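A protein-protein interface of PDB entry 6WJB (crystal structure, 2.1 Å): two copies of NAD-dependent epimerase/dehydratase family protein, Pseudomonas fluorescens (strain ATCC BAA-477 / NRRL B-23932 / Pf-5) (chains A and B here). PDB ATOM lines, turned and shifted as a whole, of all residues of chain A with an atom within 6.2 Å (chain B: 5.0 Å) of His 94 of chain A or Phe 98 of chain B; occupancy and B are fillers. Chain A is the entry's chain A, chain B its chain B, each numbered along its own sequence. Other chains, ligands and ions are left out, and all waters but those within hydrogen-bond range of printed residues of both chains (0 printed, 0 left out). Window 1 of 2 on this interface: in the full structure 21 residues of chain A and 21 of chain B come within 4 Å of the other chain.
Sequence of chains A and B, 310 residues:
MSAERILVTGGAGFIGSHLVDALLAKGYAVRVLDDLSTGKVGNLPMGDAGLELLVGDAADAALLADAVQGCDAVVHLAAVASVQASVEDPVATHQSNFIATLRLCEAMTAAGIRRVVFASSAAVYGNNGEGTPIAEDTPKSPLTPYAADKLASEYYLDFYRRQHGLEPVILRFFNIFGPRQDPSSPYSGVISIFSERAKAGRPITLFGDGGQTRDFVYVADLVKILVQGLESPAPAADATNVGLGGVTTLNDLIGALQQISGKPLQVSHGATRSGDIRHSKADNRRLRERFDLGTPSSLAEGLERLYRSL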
ATOM      1  N   ASP A  89      -9.297 -14.476  -1.415  1.00  0.00           N
ATOM      2  CA  ASP A  89     -10.165 -14.593  -0.241  1.00  0.00           C
ATOM      3  C   ASP A  89      -9.320 -14.709   1.026  1.00  0.00           C
ATOM      4  O   ASP A  89      -9.209 -15.781   1.632  1.00  0.00           O
ATOM      5  CB  ASP A  89     -11.109 -15.784  -0.387  1.00  0.00           C
ATOM      6  CG  ASP A  89     -12.313 -15.684   0.533  1.00  0.00           C
ATOM      7  OD1 ASP A  89     -12.256 -14.909   1.522  1.00  0.00           O
ATOM      8  OD2 ASP A  89     -13.315 -16.377   0.257  1.00  0.00           O
ATOM      9  N   PRO A  90      -8.723 -13.599   1.468  1.00  0.00           N
ATOM     10  CA  PRO A  90      -7.873 -13.671   2.671  1.00  0.00           C
ATOM     11  C   PRO A  90      -8.627 -14.125   3.908  1.00  0.00           C
ATOM     12  O   PRO A  90      -8.070 -14.852   4.742  1.00  0.00           O
ATOM     13  CB  PRO A  90      -7.353 -12.232   2.817  1.00  0.00           C
ATOM     14  CG  PRO A  90      -7.483 -11.623   1.416  1.00  0.00           C
ATOM     15  CD  PRO A  90      -8.707 -12.269   0.833  1.00  0.00           C
ATOM     16  N   VAL A  91      -9.899 -13.734   4.033  1.00  0.00           N
ATOM     17  CA  VAL A  91     -10.658 -14.037   5.241  1.00  0.00           C
ATOM     18  C   VAL A  91     -10.903 -15.537   5.357  1.00  0.00           C
ATOM     19  O   VAL A  91     -10.593 -16.155   6.384  1.00  0.00           O
ATOM     20  CB  VAL A  91     -11.977 -13.240   5.261  1.00  0.00           C
ATOM     21  CG1 VAL A  91     -12.868 -13.721   6.395  1.00  0.00           C
ATOM     22  CG2 VAL A  91     -11.681 -11.744   5.392  1.00  0.00           C
ATOM     23  N   ALA A  92     -11.454 -16.148   4.302  1.00  0.00           N
ATOM     24  CA  ALA A  92     -11.730 -17.579   4.357  1.00  0.00           C
ATOM     25  C   ALA A  92     -10.447 -18.398   4.472  1.00  0.00           C
ATOM     26  O   ALA A  92     -10.382 -19.337   5.272  1.00  0.00           O
ATOM     27  CB  ALA A  92     -12.538 -18.009   3.128  1.00  0.00           C
ATOM     28  N   THR A  93      -9.410 -18.064   3.701  1.00  0.00           N
ATOM     29  CA  THR A  93      -8.217 -18.907   3.733  1.00  0.00           C
ATOM     30  C   THR A  93      -7.450 -18.769   5.049  1.00  0.00           C
ATOM     31  O   THR A  93      -6.777 -19.717   5.466  1.00  0.00           O
ATOM     32  CB  THR A  93      -7.295 -18.608   2.544  1.00  0.00           C
ATOM     33  OG1 THR A  93      -6.924 -17.221   2.537  1.00  0.00           O
ATOM     34  CG2 THR A  93      -7.989 -19.001   1.202  1.00  0.00           C
ATOM     35  N   HIS A  94      -7.540 -17.617   5.721  1.00  0.00           N
ATOM     36  CA  HIS A  94      -6.890 -17.490   7.030  1.00  0.00           C
ATOM     37  C   HIS A  94      -7.426 -18.513   8.037  1.00  0.00           C
ATOM     38  O   HIS A  94      -6.670 -18.993   8.885  1.00  0.00           O
ATOM     39  CB  HIS A  94      -7.052 -16.059   7.564  1.00  0.00           C
ATOM     40  CG  HIS A  94      -6.514 -15.854   8.949  1.00  0.00           C
ATOM     41  ND1 HIS A  94      -5.168 -15.712   9.214  1.00  0.00           N
ATOM     42  CD2 HIS A  94      -7.145 -15.748  10.146  1.00  0.00           C
ATOM     43  CE1 HIS A  94      -4.990 -15.533  10.513  1.00  0.00           C
ATOM     44  NE2 HIS A  94      -6.174 -15.547  11.101  1.00  0.00           N
ATOM     45  N   GLN A  95      -8.720 -18.854   7.972  1.00  0.00           N
ATOM     46  CA  GLN A  95      -9.250 -19.920   8.830  1.00  0.00           C
ATOM     47  C   GLN A  95      -8.506 -21.232   8.604  1.00  0.00           C
ATOM     48  O   GLN A  95      -8.119 -21.915   9.558  1.00  0.00           O
ATOM     49  CB  GLN A  95     -10.747 -20.139   8.557  1.00  0.00           C
ATOM     50  CG  GLN A  95     -11.600 -18.972   8.890  1.00  0.00           C
ATOM     51  CD  GLN A  95     -11.662 -18.746  10.381  1.00  0.00           C
ATOM     52  OE1 GLN A  95     -11.198 -17.719  10.886  1.00  0.00           O
ATOM     53  NE2 GLN A  95     -12.227 -19.713  11.099  1.00  0.00           N
ATOM     54  N   SER A  96      -8.346 -21.621   7.340  1.00  0.00           N
ATOM     55  CA  SER A  96      -7.683 -22.882   7.020  1.00  0.00           C
ATOM     56  C   SER A  96      -6.174 -22.793   7.205  1.00  0.00           C
ATOM     57  O   SER A  96      -5.537 -23.765   7.635  1.00  0.00           O
ATOM     58  CB  SER A  96      -8.013 -23.293   5.584  1.00  0.00           C
ATOM     59  OG  SER A  96      -9.369 -23.720   5.481  1.00  0.00           O
ATOM     60  N   ASN A  97      -5.574 -21.647   6.876  1.00  0.00           N
ATOM     61  CA  ASN A  97      -4.117 -21.573   6.821  1.00  0.00           C
ATOM     62  C   ASN A  97      -3.487 -21.119   8.133  1.00  0.00           C
ATOM     63  O   ASN A  97      -2.280 -21.322   8.327  1.00  0.00           O
ATOM     64  CB  ASN A  97      -3.667 -20.635   5.685  1.00  0.00           C
ATOM     65  CG  ASN A  97      -4.069 -21.152   4.308  1.00  0.00           C
ATOM     66  OD1 ASN A  97      -4.322 -22.340   4.138  1.00  0.00           O
ATOM     67  ND2 ASN A  97      -4.120 -20.257   3.320  1.00  0.00           N
ATOM     68  N   PHE A  98      -4.256 -20.513   9.035  1.00  0.00           N
ATOM     69  CA  PHE A  98      -3.694 -20.201  10.344  1.00  0.00           C
ATOM     70  C   PHE A  98      -4.563 -20.689  11.493  1.00  0.00           C
ATOM     71  O   PHE A  98      -4.047 -21.297  12.439  1.00  0.00           O
ATOM     72  CB  PHE A  98      -3.457 -18.699  10.547  1.00  0.00           C
ATOM     73  CG  PHE A  98      -3.106 -18.363  11.983  1.00  0.00           C
ATOM     74  CD1 PHE A  98      -1.820 -18.574  12.456  1.00  0.00           C
ATOM     75  CD2 PHE A  98      -4.077 -17.921  12.868  1.00  0.00           C
ATOM     76  CE1 PHE A  98      -1.492 -18.315  13.783  1.00  0.00           C
ATOM     77  CE2 PHE A  98      -3.766 -17.663  14.207  1.00  0.00           C
ATOM     78  CZ  PHE A  98      -2.466 -17.851  14.660  1.00  0.00           C
ATOM     79  N   ILE A  99      -5.871 -20.401  11.450  1.00  0.00           N
ATOM     80  CA  ILE A  99      -6.720 -20.715  12.601  1.00  0.00           C
ATOM     81  C   ILE A  99      -6.679 -22.207  12.898  1.00  0.00           C
ATOM     82  O   ILE A  99      -6.650 -22.628  14.065  1.00  0.00           O
ATOM     83  CB  ILE A  99      -8.154 -20.221  12.367  1.00  0.00           C
ATOM     84  CG1 ILE A  99      -8.157 -18.703  12.169  1.00  0.00           C
ATOM     85  CG2 ILE A  99      -9.051 -20.606  13.566  1.00  0.00           C
ATOM     86  CD1 ILE A  99      -7.883 -17.929  13.453  1.00  0.00           C
ATOM     87  N   ALA A 100      -6.646 -23.027  11.846  1.00  0.00           N
ATOM     88  CA  ALA A 100      -6.493 -24.466  12.028  1.00  0.00           C
ATOM     89  C   ALA A 100      -5.248 -24.792  12.852  1.00  0.00           C
ATOM     90  O   ALA A 100      -5.300 -25.631  13.757  1.00  0.00           O
ATOM     91  CB  ALA A 100      -6.440 -25.158  10.663  1.00  0.00           C
ATOM     92  N   PRO A 145      -1.500 -13.572   1.901  1.00  0.00           N
ATOM     93  CA  PRO A 145      -2.074 -14.132   3.141  1.00  0.00           C
ATOM     94  C   PRO A 145      -1.588 -15.546   3.437  1.00  0.00           C
ATOM     95  O   PRO A 145      -1.301 -15.865   4.594  1.00  0.00           O
ATOM     96  CB  PRO A 145      -3.592 -14.103   2.867  1.00  0.00           C
ATOM     97  CG  PRO A 145      -3.781 -12.948   1.909  1.00  0.00           C
ATOM     98  CD  PRO A 145      -2.545 -13.042   0.999  1.00  0.00           C
ATOM     99  N   ASP A 149       0.314 -16.506   6.786  1.00  0.00           N
ATOM    100  CA  ASP A 149      -0.320 -17.456   7.697  1.00  0.00           C
ATOM    101  C   ASP A 149       0.602 -18.625   8.014  1.00  0.00           C
ATOM    102  O   ASP A 149       0.603 -19.136   9.141  1.00  0.00           O
ATOM    103  CB  ASP A 149      -1.618 -17.988   7.087  1.00  0.00           C
ATOM    104  CG  ASP A 149      -2.750 -16.978   7.131  1.00  0.00           C
ATOM    105  OD1 ASP A 149      -2.600 -15.883   7.735  1.00  0.00           O
ATOM    106  OD2 ASP A 149      -3.799 -17.293   6.551  1.00  0.00           O
ATOM    107  N   ALA A 152       3.031 -17.116  10.511  1.00  0.00           N
ATOM    108  CA  ALA A 152       2.371 -16.929  11.805  1.00  0.00           C
ATOM    109  C   ALA A 152       2.138 -18.269  12.498  1.00  0.00           C
ATOM    110  O   ALA A 152       2.316 -18.391  13.717  1.00  0.00           O
ATOM    111  CB  ALA A 152       1.050 -16.178  11.620  1.00  0.00           C
ATOM    112  N   THR B  93      -7.742 -13.341  22.021  1.00  0.00           N
ATOM    113  CA  THR B  93      -6.983 -12.145  21.673  1.00  0.00           C
ATOM    114  C   THR B  93      -6.612 -12.115  20.194  1.00  0.00           C
ATOM    115  O   THR B  93      -6.451 -11.027  19.628  1.00  0.00           O
ATOM    116  CB  THR B  93      -5.723 -12.020  22.542  1.00  0.00           C
ATOM    117  OG1 THR B  93      -4.914 -13.190  22.408  1.00  0.00           O
ATOM    118  CG2 THR B  93      -6.099 -11.829  24.012  1.00  0.00           C
ATOM    119  N   HIS B  94      -6.475 -13.277  19.545  1.00  0.00           N
ATOM    120  CA  HIS B  94      -6.174 -13.250  18.111  1.00  0.00           C
ATOM    121  C   HIS B  94      -7.281 -12.547  17.328  1.00  0.00           C
ATOM    122  O   HIS B  94      -7.005 -11.895  16.318  1.00  0.00           O
ATOM    123  CB  HIS B  94      -5.956 -14.663  17.568  1.00  0.00           C
ATOM    124  CG  HIS B  94      -5.685 -14.710  16.091  1.00  0.00           C
ATOM    125  ND1 HIS B  94      -4.464 -14.369  15.546  1.00  0.00           N
ATOM    126  CD2 HIS B  94      -6.475 -15.067  15.046  1.00  0.00           C
ATOM    127  CE1 HIS B  94      -4.514 -14.502  14.230  1.00  0.00           C
ATOM    128  NE2 HIS B  94      -5.722 -14.930  13.901  1.00  0.00           N
ATOM    129  N   GLN B  95      -8.528 -12.642  17.792  1.00  0.00           N
ATOM    130  CA  GLN B  95      -9.623 -11.914  17.151  1.00  0.00           C
ATOM    131  C   GLN B  95      -9.395 -10.410  17.214  1.00  0.00           C
ATOM    132  O   GLN B  95      -9.573  -9.699  16.219  1.00  0.00           O
ATOM    133  CB  GLN B  95     -10.956 -12.262  17.825  1.00  0.00           C
ATOM    134  CG  GLN B  95     -11.391 -13.694  17.644  1.00  0.00           C
ATOM    135  CD  GLN B  95     -11.743 -14.005  16.204  1.00  0.00           C
ATOM    136  OE1 GLN B  95     -12.537 -13.296  15.588  1.00  0.00           O
ATOM    137  NE2 GLN B  95     -11.144 -15.060  15.656  1.00  0.00           N
ATOM    138  N   SER B  96      -9.049  -9.904  18.398  1.00  0.00           N
ATOM    139  CA  SER B  96      -8.818  -8.475  18.568  1.00  0.00           C
ATOM    140  C   SER B  96      -7.471  -8.031  18.000  1.00  0.00           C
ATOM    141  O   SER B  96      -7.355  -6.917  17.478  1.00  0.00           O
ATOM    142  CB  SER B  96      -8.910  -8.118  20.049  1.00  0.00           C
ATOM    143  OG  SER B  96     -10.233  -8.318  20.554  1.00  0.00           O
ATOM    144  N   ASN B  97      -6.449  -8.870  18.083  1.00  0.00           N
ATOM    145  CA  ASN B  97      -5.107  -8.423  17.733  1.00  0.00           C
ATOM    146  C   ASN B  97      -4.752  -8.655  16.275  1.00  0.00           C
ATOM    147  O   ASN B  97      -3.778  -8.064  15.789  1.00  0.00           O
ATOM    148  CB  ASN B  97      -4.078  -9.115  18.630  1.00  0.00           C
ATOM    149  CG  ASN B  97      -4.245  -8.722  20.081  1.00  0.00           C
ATOM    150  OD1 ASN B  97      -4.888  -7.715  20.372  1.00  0.00           O
ATOM    151  ND2 ASN B  97      -3.671  -9.503  20.991  1.00  0.00           N
ATOM    152  N   PHE B  98      -5.501  -9.499  15.567  1.00  0.00           N
ATOM    153  CA  PHE B  98      -5.209  -9.671  14.151  1.00  0.00           C
ATOM    154  C   PHE B  98      -6.456  -9.623  13.281  1.00  0.00           C
ATOM    155  O   PHE B  98      -6.460  -8.941  12.253  1.00  0.00           O
ATOM    156  CB  PHE B  98      -4.488 -10.981  13.854  1.00  0.00           C
ATOM    157  CG  PHE B  98      -4.424 -11.253  12.392  1.00  0.00           C
ATOM    158  CD1 PHE B  98      -3.511 -10.569  11.598  1.00  0.00           C
ATOM    159  CD2 PHE B  98      -5.340 -12.090  11.786  1.00  0.00           C
ATOM    160  CE1 PHE B  98      -3.474 -10.769  10.224  1.00  0.00           C
ATOM    161  CE2 PHE B  98      -5.314 -12.280  10.412  1.00  0.00           C
ATOM    162  CZ  PHE B  98      -4.372 -11.628   9.637  1.00  0.00           C
ATOM    163  N   ILE B  99      -7.498 -10.373  13.650  1.00  0.00           N
ATOM    164  CA  ILE B  99      -8.692 -10.433  12.808  1.00  0.00           C
ATOM    165  C   ILE B  99      -9.270  -9.036  12.598  1.00  0.00           C
ATOM    166  O   ILE B  99      -9.686  -8.683  11.489  1.00  0.00           O
ATOM    167  CB  ILE B  99      -9.723 -11.400  13.413  1.00  0.00           C
ATOM    168  CG1 ILE B  99      -9.107 -12.798  13.567  1.00  0.00           C
ATOM    169  CG2 ILE B  99     -10.982 -11.444  12.559  1.00  0.00           C
ATOM    170  CD1 ILE B  99      -9.127 -13.630  12.305  1.00  0.00           C
ATOM    171  N   ALA B 100      -9.285  -8.214  13.652  1.00  0.00           N
ATOM    172  CA  ALA B 100      -9.725  -6.828  13.504  1.00  0.00           C
ATOM    173  C   ALA B 100      -8.952  -6.102  12.400  1.00  0.00           C
ATOM    174  O   ALA B 100      -9.535  -5.341  11.621  1.00  0.00           O
ATOM    175  CB  ALA B 100      -9.560  -6.086  14.826  1.00  0.00           C
ATOM    176  N   THR B 101      -7.636  -6.320  12.320  1.00  0.00           N
ATOM    177  CA  THR B 101      -6.844  -5.695  11.259  1.00  0.00           C
ATOM    178  C   THR B 101      -7.276  -6.204   9.887  1.00  0.00           C
ATOM    179  O   THR B 101      -7.466  -5.423   8.945  1.00  0.00           O
ATOM    180  CB  THR B 101      -5.353  -5.965  11.480  1.00  0.00           C
ATOM    181  OG1 THR B 101      -4.929  -5.386  12.722  1.00  0.00           O
ATOM    182  CG2 THR B 101      -4.507  -5.382  10.336  1.00  0.00           C
ATOM    183  N   LEU B 102      -7.419  -7.522   9.755  1.00  0.00           N
ATOM    184  CA  LEU B 102      -7.836  -8.111   8.486  1.00  0.00           C
ATOM    185  C   LEU B 102      -9.216  -7.609   8.065  1.00  0.00           C
ATOM    186  O   LEU B 102      -9.428  -7.222   6.909  1.00  0.00           O
ATOM    187  CB  LEU B 102      -7.822  -9.633   8.609  1.00  0.00           C
ATOM    188  CG  LEU B 102      -8.444 -10.458   7.479  1.00  0.00           C
ATOM    189  CD1 LEU B 102      -7.851 -10.086   6.128  1.00  0.00           C
ATOM    190  CD2 LEU B 102      -8.222 -11.942   7.769  1.00  0.00           C
ATOM    191  N   ASP B 149       0.688 -11.440  16.263  1.00  0.00           N
ATOM    192  CA  ASP B 149      -0.479 -10.853  15.610  1.00  0.00           C
ATOM    193  C   ASP B 149      -0.185  -9.449  15.115  1.00  0.00           C
ATOM    194  O   ASP B 149      -0.712  -9.030  14.076  1.00  0.00           O
ATOM    195  CB  ASP B 149      -1.670 -10.820  16.574  1.00  0.00           C
ATOM    196  CG  ASP B 149      -2.281 -12.190  16.800  1.00  0.00           C
ATOM    197  OD1 ASP B 149      -1.912 -13.161  16.091  1.00  0.00           O
ATOM    198  OD2 ASP B 149      -3.132 -12.290  17.701  1.00  0.00           O
ATOM    199  N   ALA B 152       1.903 -10.148  12.016  1.00  0.00           N
ATOM    200  CA  ALA B 152       1.000 -10.625  10.971  1.00  0.00           C
ATOM    201  C   ALA B 152       0.138  -9.488  10.433  1.00  0.00           C
ATOM    202  O   ALA B 152      -0.099  -9.391   9.218  1.00  0.00           O
ATOM    203  CB  ALA B 152       0.128 -11.753  11.517  1.00  0.00           C
ATOM    204  N   SER B 153      -0.347  -8.618  11.326  1.00  0.00           N
ATOM    205  CA  SER B 153      -1.073  -7.429  10.892  1.00  0.00           C
ATOM    206  C   SER B 153      -0.245  -6.596   9.920  1.00  0.00           C
ATOM    207  O   SER B 153      -0.773  -6.113   8.912  1.00  0.00           O
ATOM    208  CB  SER B 153      -1.478  -6.569  12.095  1.00  0.00           C
ATOM    209  OG  SER B 153      -2.514  -7.170  12.864  1.00  0.00           O
ATOM    210  N   TYR B 156      -0.170  -8.389   6.468  1.00  0.00           N
ATOM    211  CA  TYR B 156      -1.420  -8.257   5.723  1.00  0.00           C
ATOM    212  C   TYR B 156      -1.625  -6.832   5.229  1.00  0.00           C
ATOM    213  O   TYR B 156      -2.137  -6.626   4.122  1.00  0.00           O
ATOM    214  CB  TYR B 156      -2.603  -8.690   6.586  1.00  0.00           C
ATOM    215  CG  TYR B 156      -2.941 -10.164   6.484  1.00  0.00           C
ATOM    216  CD1 TYR B 156      -2.111 -11.134   7.050  1.00  0.00           C
ATOM    217  CD2 TYR B 156      -4.096 -10.585   5.832  1.00  0.00           C
ATOM    218  CE1 TYR B 156      -2.427 -12.489   6.966  1.00  0.00           C
ATOM    219  CE2 TYR B 156      -4.420 -11.943   5.734  1.00  0.00           C
ATOM    220  CZ  TYR B 156      -3.587 -12.883   6.309  1.00  0.00           C
ATOM    221  OH  TYR B 156      -3.909 -14.216   6.224  1.00  0.00           O
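The backbone carbonyl oxygen (O) of His 94 of chain B sits at hydrogen-bond distance from the backbone NH (N) of Ile 99 of chain B, at 3.1 Å. O of Pro 90 of chain A lies within hydrogen-bond range of OG1 of Thr 93 of chain A (3.4 Å). OD1 of Asp 149 of chain B lies within hydrogen-bond range of ND1 of His 94 of chain B (2.9 Å). The side-chain carboxylate (OD1) of Asp 149 of chain A lies within hydrogen-bond range of a ring nitrogen (ND1) of His 94 of chain A (3.0 Å). The backbone carbonyl oxygen (O) of His 94 of chain A sits at hydrogen-bond distance from the backbone NH (N) of Ile 99 of chain A (3.0 Å).
OH of Tyr 156 of chain B sits close to O of Pro 145 of chain A (3.5 Å). NE2 of His 94 of chain B sits at hydrogen-bond distance from NE2 of His 94 of chain A (2.9 Å). The side-chain hydroxyl of Tyr 156 of chain B lies within hydrogen-bond range of the side-chain carboxylate of Asp 149 of chain A (2.6 Å).
Gln 95 of chain A touches none of the printed residues of chain B. Of the printed residues of chain B, Pro 145 of chain A touches Tyr 156. Printed residues of chain A within 4 Å of Leu 102 of chain B: Pro 90.
Printed residues of chain B that touch a printed residue of chain A: His 94, Phe 98, Ile 99, Leu 102 and Tyr 156. Hydrophobic or aromatic side chains of chain B within 4 Å of the printed part of chain A: His 94, Phe 98, Ile 99, Leu 102 and Tyr 156. Hydrophobic or aromatic side chains of chain A that line the printed part of chain B: Pro 90, His 94, Phe 98, Ile 99 and Pro 145. Among the printed residues, 9 pairs touch across the chains. Among the printed residues, no Asp or Glu carboxylate lies within 4 Å of a Lys or Arg side-chain nitrogen of the other chain.
Among the printed residues, pairs that only touch across the chains: Phe 98 of chain A with His 94 of chain B (3.2 Å), His 94 of chain A with Phe 98 of chain B (3.3 Å), Ile 99 of chain A with His 94 of chain B (3.6 Å), His 94 of chain A with Tyr 156 of chain B (3.6 Å), His 94 of chain A with Ile 99 of chain B (3.6 Å) and Pro 90 of chain A with Leu 102 of chain B (3.98 Å).
His 94 of chain B touches its own counterpart, His 94 of chain A. His 94 of chain A touches Phe 98 of chain B, and with the chains exchanged Phe 98 of chain A touches His 94 of chain B. His 94 of chain A touches Ile 99 of chain B, and with the chains exchanged Ile 99 of chain A touches His 94 of chain B. Of the 9 pairs that touch across the chains among the printed residues, 5 have their exchanged pair printed and touching as well.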
